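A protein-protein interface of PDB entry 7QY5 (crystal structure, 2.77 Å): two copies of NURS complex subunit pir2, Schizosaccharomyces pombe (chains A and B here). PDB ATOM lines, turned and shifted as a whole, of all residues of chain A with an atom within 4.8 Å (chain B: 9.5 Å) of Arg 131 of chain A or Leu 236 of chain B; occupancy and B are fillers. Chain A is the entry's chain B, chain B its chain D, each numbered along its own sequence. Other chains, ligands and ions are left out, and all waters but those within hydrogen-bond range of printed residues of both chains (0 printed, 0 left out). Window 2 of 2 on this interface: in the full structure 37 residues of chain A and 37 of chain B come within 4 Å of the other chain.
Asp 130 of chain A touches none of the printed residues of chain B.
Of chain B, only Leu 236 (3.0 Å) and Leu 237 (3.7 Å) come within 4 Å of Arg 131 of chain A.
No residue of chain B comes within 4 Å of Ala 132 of chain A.
No residue of chain B comes within 4 Å of Ser 133 of chain A.
No residue of chain B comes within 4 Å of Thr 134 of chain A.
Asp 228 of chain B touches none of the printed residues of chain A.
Of the printed residues of chain A, Phe 233 of chain B touches Phe 128 (3.7 Å) and Ser 190 (3.5 Å).
Printed residues of chain A within 4 Å of Leu 236 of chain B: Phe 128 (3.9 Å), Arg 131 (3.0 Å), Phe 185 (3.99 Å) and Ser 190 (3.1 Å).
Of the printed residues of chain A, Glu 238 of chain B touches Arg 127 (3.7 Å).
Of the printed residues of chain A, Pro 318 of chain B touches Ser 190 (3.3 Å).
The nearest residue of chain B that does not touch Arg 131 of chain A is Cys 235 of chain B (6.4 Å).
No position is printed for both chains.
Of the 13 pairs that touch across the chains among the printed residues, none has its exchanged pair printed and touching as well.
OE1 of Glu 238 of chain B lies within salt-bridge range of NH1 of Arg 127 of chain A (3.7 Å).
The guanidinium group (NH1) of Arg 131 of chain A sits at hydrogen-bond distance from the backbone carbonyl oxygen (O) of Leu 236 of chain B, 3.0 Å away.
Leu 237 of chain B touches Arg 127 of chain A.
Phe 128 of chain A touches Phe 233 of chain B.
CD1 of Leu 236 of chain B touches CE1 of Phe 128 of chain A (3.9 Å).
CD2 of Leu 237 of chain B touches CE1 of Phe 128 of chain A, at 3.8 Å.
CD2 of Leu 237 of chain B touches CD of Arg 131 of chain A (3.7 Å).
Leu 236 of chain B touches Phe 185 of chain A.
CB of Ser 190 of chain A touches CB of Asn 232 of chain B, at 3.6 Å.
Ser 190 of chain A touches Phe 233 of chain B (CB to CE1, 3.5 Å).
Pro 318 of chain B touches Ser 190 of chain A.
SG of Cys 319 of chain B touches O of Ser 190 of chain A, at 3.9 Å.
The side-chain amide nitrogen (ND2) of Asn 232 of chain B lies within hydrogen-bond range of the backbone carbonyl oxygen (O) of Asp 228 of chain B (3.2 Å).
OE2 of Glu 192 of chain A is in salt-bridge range of NH2 of Arg 131 of chain A, at 3.0 Å.
The side-chain hydroxyl of Thr 134 of chain A is in hydrogen-bond range of the backbone carbonyl oxygen of Arg 131 of chain A, 3.0 Å away.
OD1 of Asp 317 of chain B lies within hydrogen-bond range of N of Cys 319 of chain B.
Printed residues of chain A that touch a printed residue of chain B: Arg 127, Phe 128, Arg 131, Phe 185 and Ser 190.
Hydrophobic or aromatic side chains of chain A that line the printed part of chain B: Phe 128 and Phe 185.
Hydrophobic or aromatic side chains of chain B that line the printed part of chain A: Phe 233, Leu 236, Leu 237 and Pro 318.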
ATOM      1  N   ARG A 127     -23.372   2.291  24.695  1.00  0.00           N
ATOM      2  CA  ARG A 127     -22.514   2.733  23.563  1.00  0.00           C
ATOM      3  C   ARG A 127     -22.680   4.237  23.320  1.00  0.00           C
ATOM      4  O   ARG A 127     -21.733   4.842  22.812  1.00  0.00           O
ATOM      5  CB  ARG A 127     -22.834   1.943  22.293  1.00  0.00           C
ATOM      6  CG  ARG A 127     -22.316   0.514  22.306  1.00  0.00           C
ATOM      7  CD  ARG A 127     -22.371  -0.109  20.934  1.00  0.00           C
ATOM      8  NE  ARG A 127     -21.463   0.584  20.032  1.00  0.00           N
ATOM      9  CZ  ARG A 127     -21.377   0.360  18.724  1.00  0.00           C
ATOM     10  NH1 ARG A 127     -22.146  -0.553  18.150  1.00  0.00           N
ATOM     11  NH2 ARG A 127     -20.519   1.047  17.990  1.00  0.00           N
ATOM     12  N   PHE A 128     -23.829   4.818  23.671  1.00  0.00           N
ATOM     13  CA  PHE A 128     -24.129   6.262  23.468  1.00  0.00           C
ATOM     14  C   PHE A 128     -23.583   7.083  24.643  1.00  0.00           C
ATOM     15  O   PHE A 128     -23.129   8.232  24.425  1.00  0.00           O
ATOM     16  CB  PHE A 128     -25.632   6.493  23.258  1.00  0.00           C
ATOM     17  CG  PHE A 128     -26.104   6.315  21.835  1.00  0.00           C
ATOM     18  CD1 PHE A 128     -25.542   7.056  20.802  1.00  0.00           C
ATOM     19  CD2 PHE A 128     -27.119   5.423  21.524  1.00  0.00           C
ATOM     20  CE1 PHE A 128     -25.972   6.893  19.494  1.00  0.00           C
ATOM     21  CE2 PHE A 128     -27.555   5.272  20.216  1.00  0.00           C
ATOM     22  CZ  PHE A 128     -26.979   6.004  19.204  1.00  0.00           C
ATOM     23  N   ILE A 129     -23.646   6.527  25.853  1.00  0.00           N
ATOM     24  CA  ILE A 129     -22.982   7.108  27.052  1.00  0.00           C
ATOM     25  C   ILE A 129     -21.502   7.298  26.697  1.00  0.00           C
ATOM     26  O   ILE A 129     -21.009   8.432  26.827  1.00  0.00           O
ATOM     27  CB  ILE A 129     -23.218   6.214  28.286  1.00  0.00           C
ATOM     28  CG1 ILE A 129     -24.670   6.308  28.758  1.00  0.00           C
ATOM     29  CG2 ILE A 129     -22.255   6.536  29.417  1.00  0.00           C
ATOM     30  CD1 ILE A 129     -25.115   5.171  29.648  1.00  0.00           C
ATOM     31  N   ASP A 130     -20.854   6.248  26.192  1.00  0.00           N
ATOM     32  CA  ASP A 130     -19.395   6.220  25.903  1.00  0.00           C
ATOM     33  C   ASP A 130     -19.094   7.153  24.726  1.00  0.00           C
ATOM     34  O   ASP A 130     -18.041   7.849  24.755  1.00  0.00           O
ATOM     35  CB  ASP A 130     -18.919   4.784  25.678  1.00  0.00           C
ATOM     36  CG  ASP A 130     -19.153   3.894  26.894  1.00  0.00           C
ATOM     37  OD1 ASP A 130     -19.899   4.327  27.812  1.00  0.00           O
ATOM     38  OD2 ASP A 130     -18.594   2.773  26.929  1.00  0.00           O
ATOM     39  N   ARG A 131     -19.991   7.201  23.742  1.00  0.00           N
ATOM     40  CA  ARG A 131     -19.859   8.113  22.579  1.00  0.00           C
ATOM     41  C   ARG A 131     -19.888   9.563  23.075  1.00  0.00           C
ATOM     42  O   ARG A 131     -19.105  10.396  22.554  1.00  0.00           O
ATOM     43  CB  ARG A 131     -20.979   7.831  21.582  1.00  0.00           C
ATOM     44  CG  ARG A 131     -20.961   8.713  20.343  1.00  0.00           C
ATOM     45  CD  ARG A 131     -22.107   8.341  19.434  1.00  0.00           C
ATOM     46  NE  ARG A 131     -22.733   9.513  18.859  1.00  0.00           N
ATOM     47  CZ  ARG A 131     -22.358  10.087  17.722  1.00  0.00           C
ATOM     48  NH1 ARG A 131     -21.339   9.611  17.020  1.00  0.00           N
ATOM     49  NH2 ARG A 131     -23.010  11.151  17.288  1.00  0.00           N
ATOM     50  N   ALA A 132     -20.752   9.851  24.050  1.00  0.00           N
ATOM     51  CA  ALA A 132     -20.918  11.195  24.646  1.00  0.00           C
ATOM     52  C   ALA A 132     -19.652  11.579  25.425  1.00  0.00           C
ATOM     53  O   ALA A 132     -19.255  12.751  25.356  1.00  0.00           O
ATOM     54  CB  ALA A 132     -22.147  11.220  25.513  1.00  0.00           C
ATOM     55  N   SER A 133     -19.015  10.628  26.106  1.00  0.00           N
ATOM     56  CA  SER A 133     -17.804  10.880  26.934  1.00  0.00           C
ATOM     57  C   SER A 133     -16.611  11.284  26.061  1.00  0.00           C
ATOM     58  O   SER A 133     -15.796  12.091  26.533  1.00  0.00           O
ATOM     59  CB  SER A 133     -17.423   9.693  27.751  1.00  0.00           C
ATOM     60  OG  SER A 133     -16.321   9.038  27.138  1.00  0.00           O
ATOM     61  N   THR A 134     -16.450  10.680  24.880  1.00  0.00           N
ATOM     62  CA  THR A 134     -15.349  11.030  23.945  1.00  0.00           C
ATOM     63  C   THR A 134     -15.720  12.355  23.276  1.00  0.00           C
ATOM     64  O   THR A 134     -14.905  13.280  23.304  1.00  0.00           O
ATOM     65  CB  THR A 134     -15.067   9.916  22.931  1.00  0.00           C
ATOM     66  OG1 THR A 134     -16.237   9.773  22.130  1.00  0.00           O
ATOM     67  CG2 THR A 134     -14.706   8.593  23.569  1.00  0.00           C
ATOM     68  N   LYS A 135     -16.927  12.451  22.732  1.00  0.00           N
ATOM     69  CA  LYS A 135     -17.366  13.647  21.969  1.00  0.00           C
ATOM     70  C   LYS A 135     -17.209  14.910  22.823  1.00  0.00           C
ATOM     71  O   LYS A 135     -16.547  15.868  22.371  1.00  0.00           O
ATOM     72  CB  LYS A 135     -18.823  13.496  21.528  1.00  0.00           C
ATOM     73  CG  LYS A 135     -19.369  14.692  20.767  1.00  0.00           C
ATOM     74  CD  LYS A 135     -20.570  14.352  19.922  1.00  0.00           C
ATOM     75  CE  LYS A 135     -21.026  15.521  19.072  1.00  0.00           C
ATOM     76  NZ  LYS A 135     -22.381  15.292  18.513  1.00  0.00           N
ATOM     77  N   PHE A 185     -29.749  14.063  24.187  1.00  0.00           N
ATOM     78  CA  PHE A 185     -29.913  13.006  23.159  1.00  0.00           C
ATOM     79  C   PHE A 185     -31.209  12.250  23.444  1.00  0.00           C
ATOM     80  O   PHE A 185     -31.335  11.708  24.572  1.00  0.00           O
ATOM     81  CB  PHE A 185     -28.679  12.106  23.155  1.00  0.00           C
ATOM     82  CG  PHE A 185     -28.707  11.044  22.095  1.00  0.00           C
ATOM     83  CD1 PHE A 185     -29.032   9.743  22.417  1.00  0.00           C
ATOM     84  CD2 PHE A 185     -28.452  11.362  20.774  1.00  0.00           C
ATOM     85  CE1 PHE A 185     -29.057   8.768  21.440  1.00  0.00           C
ATOM     86  CE2 PHE A 185     -28.494  10.389  19.793  1.00  0.00           C
ATOM     87  CZ  PHE A 185     -28.787   9.091  20.133  1.00  0.00           C
ATOM     88  N   SER A 190     -33.477   8.697  18.201  1.00  0.00           N
ATOM     89  CA  SER A 190     -32.052   8.790  17.783  1.00  0.00           C
ATOM     90  C   SER A 190     -31.715  10.202  17.304  1.00  0.00           C
ATOM     91  O   SER A 190     -30.939  10.310  16.340  1.00  0.00           O
ATOM     92  CB  SER A 190     -31.724   7.820  16.691  1.00  0.00           C
ATOM     93  OG  SER A 190     -30.346   7.934  16.354  1.00  0.00           O
ATOM     94  N   GLU A 192     -29.804  13.682  18.185  1.00  0.00           N
ATOM     95  CA  GLU A 192     -28.919  14.545  19.007  1.00  0.00           C
ATOM     96  C   GLU A 192     -29.516  15.947  18.900  1.00  0.00           C
ATOM     97  O   GLU A 192     -30.153  16.209  17.890  1.00  0.00           O
ATOM     98  CB  GLU A 192     -27.457  14.431  18.553  1.00  0.00           C
ATOM     99  CG  GLU A 192     -26.434  14.508  19.691  1.00  0.00           C
ATOM    100  CD  GLU A 192     -25.287  13.506  19.581  1.00  0.00           C
ATOM    101  OE1 GLU A 192     -24.668  13.115  20.651  1.00  0.00           O
ATOM    102  OE2 GLU A 192     -25.024  13.091  18.421  1.00  0.00           O
ATOM    103  N   ASP B 228     -36.071   0.548  12.202  1.00  0.00           N
ATOM    104  CA  ASP B 228     -35.685   1.909  11.738  1.00  0.00           C
ATOM    105  C   ASP B 228     -34.816   2.548  12.820  1.00  0.00           C
ATOM    106  O   ASP B 228     -33.785   3.170  12.476  1.00  0.00           O
ATOM    107  CB  ASP B 228     -36.911   2.748  11.362  1.00  0.00           C
ATOM    108  CG  ASP B 228     -37.464   2.425   9.978  1.00  0.00           C
ATOM    109  OD1 ASP B 228     -37.054   1.375   9.383  1.00  0.00           O
ATOM    110  OD2 ASP B 228     -38.302   3.225   9.490  1.00  0.00           O
ATOM    111  N   LEU B 229     -35.197   2.358  14.083  1.00  0.00           N
ATOM    112  CA  LEU B 229     -34.488   2.980  15.216  1.00  0.00           C
ATOM    113  C   LEU B 229     -33.072   2.412  15.264  1.00  0.00           C
ATOM    114  O   LEU B 229     -32.115   3.198  15.285  1.00  0.00           O
ATOM    115  CB  LEU B 229     -35.261   2.718  16.505  1.00  0.00           C
ATOM    116  CG  LEU B 229     -34.616   3.307  17.757  1.00  0.00           C
ATOM    117  CD1 LEU B 229     -34.543   4.824  17.686  1.00  0.00           C
ATOM    118  CD2 LEU B 229     -35.369   2.863  18.994  1.00  0.00           C
ATOM    119  N   GLU B 230     -32.935   1.091  15.238  1.00  0.00           N
ATOM    120  CA  GLU B 230     -31.601   0.433  15.286  1.00  0.00           C
ATOM    121  C   GLU B 230     -30.789   0.877  14.053  1.00  0.00           C
ATOM    122  O   GLU B 230     -29.556   1.047  14.173  1.00  0.00           O
ATOM    123  CB  GLU B 230     -31.759  -1.084  15.469  1.00  0.00           C
ATOM    124  CG  GLU B 230     -32.222  -1.470  16.874  1.00  0.00           C
ATOM    125  CD  GLU B 230     -31.790  -2.843  17.377  1.00  0.00           C
ATOM    126  OE1 GLU B 230     -31.238  -2.948  18.533  1.00  0.00           O
ATOM    127  OE2 GLU B 230     -32.016  -3.823  16.618  1.00  0.00           O
ATOM    128  N   ASN B 231     -31.450   1.120  12.920  1.00  0.00           N
ATOM    129  CA  ASN B 231     -30.769   1.562  11.676  1.00  0.00           C
ATOM    130  C   ASN B 231     -30.208   2.968  11.891  1.00  0.00           C
ATOM    131  O   ASN B 231     -29.055   3.213  11.473  1.00  0.00           O
ATOM    132  CB  ASN B 231     -31.691   1.502  10.457  1.00  0.00           C
ATOM    133  CG  ASN B 231     -31.654   0.157   9.770  1.00  0.00           C
ATOM    134  OD1 ASN B 231     -30.580  -0.395   9.530  1.00  0.00           O
ATOM    135  ND2 ASN B 231     -32.823  -0.376   9.451  1.00  0.00           N
ATOM    136  N   ASN B 232     -31.005   3.851  12.503  1.00  0.00           N
ATOM    137  CA  ASN B 232     -30.570   5.214  12.911  1.00  0.00           C
ATOM    138  C   ASN B 232     -29.327   5.111  13.808  1.00  0.00           C
ATOM    139  O   ASN B 232     -28.291   5.728  13.461  1.00  0.00           O
ATOM    140  CB  ASN B 232     -31.701   5.984  13.585  1.00  0.00           C
ATOM    141  CG  ASN B 232     -32.689   6.515  12.579  1.00  0.00           C
ATOM    142  OD1 ASN B 232     -32.281   7.088  11.574  1.00  0.00           O
ATOM    143  ND2 ASN B 232     -33.977   6.358  12.853  1.00  0.00           N
ATOM    144  N   PHE B 233     -29.391   4.337  14.893  1.00  0.00           N
ATOM    145  CA  PHE B 233     -28.240   4.194  15.818  1.00  0.00           C
ATOM    146  C   PHE B 233     -26.972   3.864  15.014  1.00  0.00           C
ATOM    147  O   PHE B 233     -25.921   4.474  15.288  1.00  0.00           O
ATOM    148  CB  PHE B 233     -28.524   3.155  16.902  1.00  0.00           C
ATOM    149  CG  PHE B 233     -29.711   3.447  17.784  1.00  0.00           C
ATOM    150  CD1 PHE B 233     -30.311   4.693  17.816  1.00  0.00           C
ATOM    151  CD2 PHE B 233     -30.221   2.465  18.616  1.00  0.00           C
ATOM    152  CE1 PHE B 233     -31.407   4.933  18.635  1.00  0.00           C
ATOM    153  CE2 PHE B 233     -31.311   2.709  19.439  1.00  0.00           C
ATOM    154  CZ  PHE B 233     -31.905   3.944  19.443  1.00  0.00           C
ATOM    155  N   ALA B 234     -27.069   2.954  14.039  1.00  0.00           N
ATOM    156  CA  ALA B 234     -25.932   2.509  13.199  1.00  0.00           C
ATOM    157  C   ALA B 234     -25.314   3.715  12.483  1.00  0.00           C
ATOM    158  O   ALA B 234     -24.079   3.826  12.452  1.00  0.00           O
ATOM    159  CB  ALA B 234     -26.384   1.459  12.221  1.00  0.00           C
ATOM    160  N   CYS B 235     -26.137   4.617  11.952  1.00  0.00           N
ATOM    161  CA  CYS B 235     -25.660   5.835  11.253  1.00  0.00           C
ATOM    162  C   CYS B 235     -24.727   6.640  12.164  1.00  0.00           C
ATOM    163  O   CYS B 235     -23.781   7.240  11.646  1.00  0.00           O
ATOM    164  CB  CYS B 235     -26.824   6.698  10.803  1.00  0.00           C
ATOM    165  SG  CYS B 235     -27.829   5.913   9.516  1.00  0.00           S
ATOM    166  N   LEU B 236     -24.980   6.637  13.473  1.00  0.00           N
ATOM    167  CA  LEU B 236     -24.205   7.421  14.470  1.00  0.00           C
ATOM    168  C   LEU B 236     -23.010   6.622  15.008  1.00  0.00           C
ATOM    169  O   LEU B 236     -21.953   7.240  15.213  1.00  0.00           O
ATOM    170  CB  LEU B 236     -25.150   7.812  15.605  1.00  0.00           C
ATOM    171  CG  LEU B 236     -26.380   8.612  15.181  1.00  0.00           C
ATOM    172  CD1 LEU B 236     -27.377   8.751  16.326  1.00  0.00           C
ATOM    173  CD2 LEU B 236     -25.969   9.978  14.663  1.00  0.00           C
ATOM    174  N   LEU B 237     -23.175   5.311  15.228  1.00  0.00           N
ATOM    175  CA  LEU B 237     -22.198   4.425  15.923  1.00  0.00           C
ATOM    176  C   LEU B 237     -21.279   3.712  14.920  1.00  0.00           C
ATOM    177  O   LEU B 237     -20.139   3.459  15.291  1.00  0.00           O
ATOM    178  CB  LEU B 237     -22.965   3.411  16.783  1.00  0.00           C
ATOM    179  CG  LEU B 237     -23.812   3.999  17.916  1.00  0.00           C
ATOM    180  CD1 LEU B 237     -24.616   2.917  18.612  1.00  0.00           C
ATOM    181  CD2 LEU B 237     -22.954   4.738  18.934  1.00  0.00           C
ATOM    182  N   GLU B 238     -21.745   3.380  13.714  1.00  0.00           N
ATOM    183  CA  GLU B 238     -20.977   2.566  12.724  1.00  0.00           C
ATOM    184  C   GLU B 238     -21.191   3.096  11.307  1.00  0.00           C
ATOM    185  O   GLU B 238     -21.418   2.312  10.384  1.00  0.00           O
ATOM    186  CB  GLU B 238     -21.433   1.099  12.697  1.00  0.00           C
ATOM    187  CG  GLU B 238     -21.509   0.402  14.043  1.00  0.00           C
ATOM    188  CD  GLU B 238     -22.446  -0.800  14.038  1.00  0.00           C
ATOM    189  OE1 GLU B 238     -22.133  -1.809  14.701  1.00  0.00           O
ATOM    190  OE2 GLU B 238     -23.501  -0.716  13.383  1.00  0.00           O
ATOM    191  N   PRO B 239     -21.135   4.424  11.063  1.00  0.00           N
ATOM    192  CA  PRO B 239     -21.404   4.951   9.726  1.00  0.00           C
ATOM    193  C   PRO B 239     -20.624   4.175   8.649  1.00  0.00           C
ATOM    194  O   PRO B 239     -21.182   3.885   7.611  1.00  0.00           O
ATOM    195  CB  PRO B 239     -20.994   6.429   9.828  1.00  0.00           C
ATOM    196  CG  PRO B 239     -20.169   6.507  11.095  1.00  0.00           C
ATOM    197  CD  PRO B 239     -20.767   5.471  12.021  1.00  0.00           C
ATOM    198  N   GLU B 240     -19.377   3.803   8.945  1.00  0.00           N
ATOM    199  CA  GLU B 240     -18.464   3.065   8.027  1.00  0.00           C
ATOM    200  C   GLU B 240     -19.050   1.697   7.633  1.00  0.00           C
ATOM    201  O   GLU B 240     -18.615   1.144   6.613  1.00  0.00           O
ATOM    202  CB  GLU B 240     -17.084   2.899   8.674  1.00  0.00           C
ATOM    203  CG  GLU B 240     -17.074   2.062   9.950  1.00  0.00           C
ATOM    204  CD  GLU B 240     -17.370   2.782  11.259  1.00  0.00           C
ATOM    205  OE1 GLU B 240     -17.451   2.095  12.300  1.00  0.00           O
ATOM    206  OE2 GLU B 240     -17.523   4.020  11.247  1.00  0.00           O
ATOM    207  N   ASN B 241     -19.979   1.147   8.420  1.00  0.00           N
ATOM    208  CA  ASN B 241     -20.580  -0.193   8.180  1.00  0.00           C
ATOM    209  C   ASN B 241     -21.975  -0.059   7.571  1.00  0.00           C
ATOM    210  O   ASN B 241     -22.610  -1.105   7.360  1.00  0.00           O
ATOM    211  CB  ASN B 241     -20.694  -0.999   9.472  1.00  0.00           C
ATOM    212  CG  ASN B 241     -19.360  -1.173  10.157  1.00  0.00           C
ATOM    213  OD1 ASN B 241     -18.312  -0.967   9.546  1.00  0.00           O
ATOM    214  ND2 ASN B 241     -19.394  -1.558  11.420  1.00  0.00           N
ATOM    215  N   VAL B 242     -22.452   1.164   7.337  1.00  0.00           N
ATOM    216  CA  VAL B 242     -23.851   1.402   6.878  1.00  0.00           C
ATOM    217  C   VAL B 242     -23.838   1.397   5.346  1.00  0.00           C
ATOM    218  O   VAL B 242     -22.813   1.797   4.775  1.00  0.00           O
ATOM    219  CB  VAL B 242     -24.433   2.694   7.491  1.00  0.00           C
ATOM    220  CG1 VAL B 242     -25.787   3.055   6.895  1.00  0.00           C
ATOM    221  CG2 VAL B 242     -24.536   2.595   9.007  1.00  0.00           C
ATOM    222  N   LYS B 247     -29.020   4.172   0.644  1.00  0.00           N
ATOM    223  CA  LYS B 247     -29.614   5.460   1.115  1.00  0.00           C
ATOM    224  C   LYS B 247     -29.488   6.560   0.054  1.00  0.00           C
ATOM    225  O   LYS B 247     -29.847   7.713   0.361  1.00  0.00           O
ATOM    226  CB  LYS B 247     -28.913   5.951   2.386  1.00  0.00           C
ATOM    227  CG  LYS B 247     -29.048   5.027   3.580  1.00  0.00           C
ATOM    228  CD  LYS B 247     -28.815   5.711   4.917  1.00  0.00           C
ATOM    229  CE  LYS B 247     -28.982   4.763   6.082  1.00  0.00           C
ATOM    230  NZ  LYS B 247     -30.207   3.938   5.918  1.00  0.00           N
ATOM    231  N   GLY B 313     -23.051  13.222   4.336  1.00  0.00           N
ATOM    232  CA  GLY B 313     -23.402  13.698   5.688  1.00  0.00           C
ATOM    233  C   GLY B 313     -24.892  13.561   5.947  1.00  0.00           C
ATOM    234  O   GLY B 313     -25.249  13.061   7.034  1.00  0.00           O
ATOM    235  N   TYR B 314     -25.719  13.984   4.978  1.00  0.00           N
ATOM    236  CA  TYR B 314     -27.200  14.146   5.065  1.00  0.00           C
ATOM    237  C   TYR B 314     -27.856  12.803   5.398  1.00  0.00           C
ATOM    238  O   TYR B 314     -28.603  12.716   6.391  1.00  0.00           O
ATOM    239  CB  TYR B 314     -27.748  14.692   3.741  1.00  0.00           C
ATOM    240  CG  TYR B 314     -29.252  14.837   3.658  1.00  0.00           C
ATOM    241  CD1 TYR B 314     -30.022  13.967   2.905  1.00  0.00           C
ATOM    242  CD2 TYR B 314     -29.914  15.872   4.303  1.00  0.00           C
ATOM    243  CE1 TYR B 314     -31.398  14.116   2.806  1.00  0.00           C
ATOM    244  CE2 TYR B 314     -31.289  16.033   4.221  1.00  0.00           C
ATOM    245  CZ  TYR B 314     -32.040  15.147   3.470  1.00  0.00           C
ATOM    246  OH  TYR B 314     -33.400  15.282   3.398  1.00  0.00           O
ATOM    247  N   VAL B 315     -27.560  11.789   4.580  1.00  0.00           N
ATOM    248  CA  VAL B 315     -28.205  10.446   4.638  1.00  0.00           C
ATOM    249  C   VAL B 315     -27.865   9.807   5.982  1.00  0.00           C
ATOM    250  O   VAL B 315     -28.743   9.124   6.523  1.00  0.00           O
ATOM    251  CB  VAL B 315     -27.800   9.550   3.452  1.00  0.00           C
ATOM    252  CG1 VAL B 315     -28.217  10.164   2.121  1.00  0.00           C
ATOM    253  CG2 VAL B 315     -26.315   9.231   3.442  1.00  0.00           C
ATOM    254  N   LEU B 316     -26.667  10.051   6.517  1.00  0.00           N
ATOM    255  CA  LEU B 316     -26.237   9.501   7.833  1.00  0.00           C
ATOM    256  C   LEU B 316     -26.813  10.330   8.993  1.00  0.00           C
ATOM    257  O   LEU B 316     -26.318  10.157  10.111  1.00  0.00           O
ATOM    258  CB  LEU B 316     -24.706   9.497   7.921  1.00  0.00           C
ATOM    259  CG  LEU B 316     -23.962   8.624   6.924  1.00  0.00           C
ATOM    260  CD1 LEU B 316     -22.474   8.635   7.223  1.00  0.00           C
ATOM    261  CD2 LEU B 316     -24.493   7.209   6.957  1.00  0.00           C
ATOM    262  N   ASP B 317     -27.778  11.218   8.760  1.00  0.00           N
ATOM    263  CA  ASP B 317     -28.358  12.042   9.852  1.00  0.00           C
ATOM    264  C   ASP B 317     -29.770  11.566  10.190  1.00  0.00           C
ATOM    265  O   ASP B 317     -30.724  11.931   9.510  1.00  0.00           O
ATOM    266  CB  ASP B 317     -28.357  13.521   9.493  1.00  0.00           C
ATOM    267  CG  ASP B 317     -28.810  14.373  10.656  1.00  0.00           C
ATOM    268  OD1 ASP B 317     -29.858  14.043  11.240  1.00  0.00           O
ATOM    269  OD2 ASP B 317     -28.096  15.336  10.982  1.00  0.00           O
ATOM    270  N   PRO B 318     -29.950  10.776  11.275  1.00  0.00           N
ATOM    271  CA  PRO B 318     -31.231  10.148  11.598  1.00  0.00           C
ATOM    272  C   PRO B 318     -32.463  11.045  11.485  1.00  0.00           C
ATOM    273  O   PRO B 318     -33.510  10.585  11.042  1.00  0.00           O
ATOM    274  CB  PRO B 318     -31.057   9.804  13.079  1.00  0.00           C
ATOM    275  CG  PRO B 318     -29.606   9.451  13.180  1.00  0.00           C
ATOM    276  CD  PRO B 318     -28.909  10.418  12.248  1.00  0.00           C
ATOM    277  N   CYS B 319     -32.308  12.283  11.940  1.00  0.00           N
ATOM    278  CA  CYS B 319     -33.398  13.279  12.076  1.00  0.00           C
ATOM    279  C   CYS B 319     -32.971  14.569  11.360  1.00  0.00           C
ATOM    280  O   CYS B 319     -33.110  15.675  11.943  1.00  0.00           O
ATOM    281  CB  CYS B 319     -33.711  13.518  13.549  1.00  0.00           C
ATOM    282  SG  CYS B 319     -34.000  12.013  14.518  1.00  0.00           S
ATOM    283  N   ARG B 320     -32.422  14.408  10.154  1.00  0.00           N
ATOM    284  CA  ARG B 320     -32.125  15.504   9.199  1.00  0.00           C
ATOM    285  C   ARG B 320     -33.417  16.248   8.891  1.00  0.00           C
ATOM    286  O   ARG B 320     -34.506  15.708   9.168  1.00  0.00           O
ATOM    287  CB  ARG B 320     -31.544  14.950   7.897  1.00  0.00           C
ATOM    288  CG  ARG B 320     -32.491  14.044   7.121  1.00  0.00           C
ATOM    289  CD  ARG B 320     -31.738  13.048   6.257  1.00  0.00           C
ATOM    290  NE  ARG B 320     -32.625  12.029   5.726  1.00  0.00           N
ATOM    291  CZ  ARG B 320     -32.837  10.838   6.273  1.00  0.00           C
ATOM    292  NH1 ARG B 320     -32.206  10.490   7.383  1.00  0.00           N
ATOM    293  NH2 ARG B 320     -33.672   9.985   5.698  1.00  0.00           N
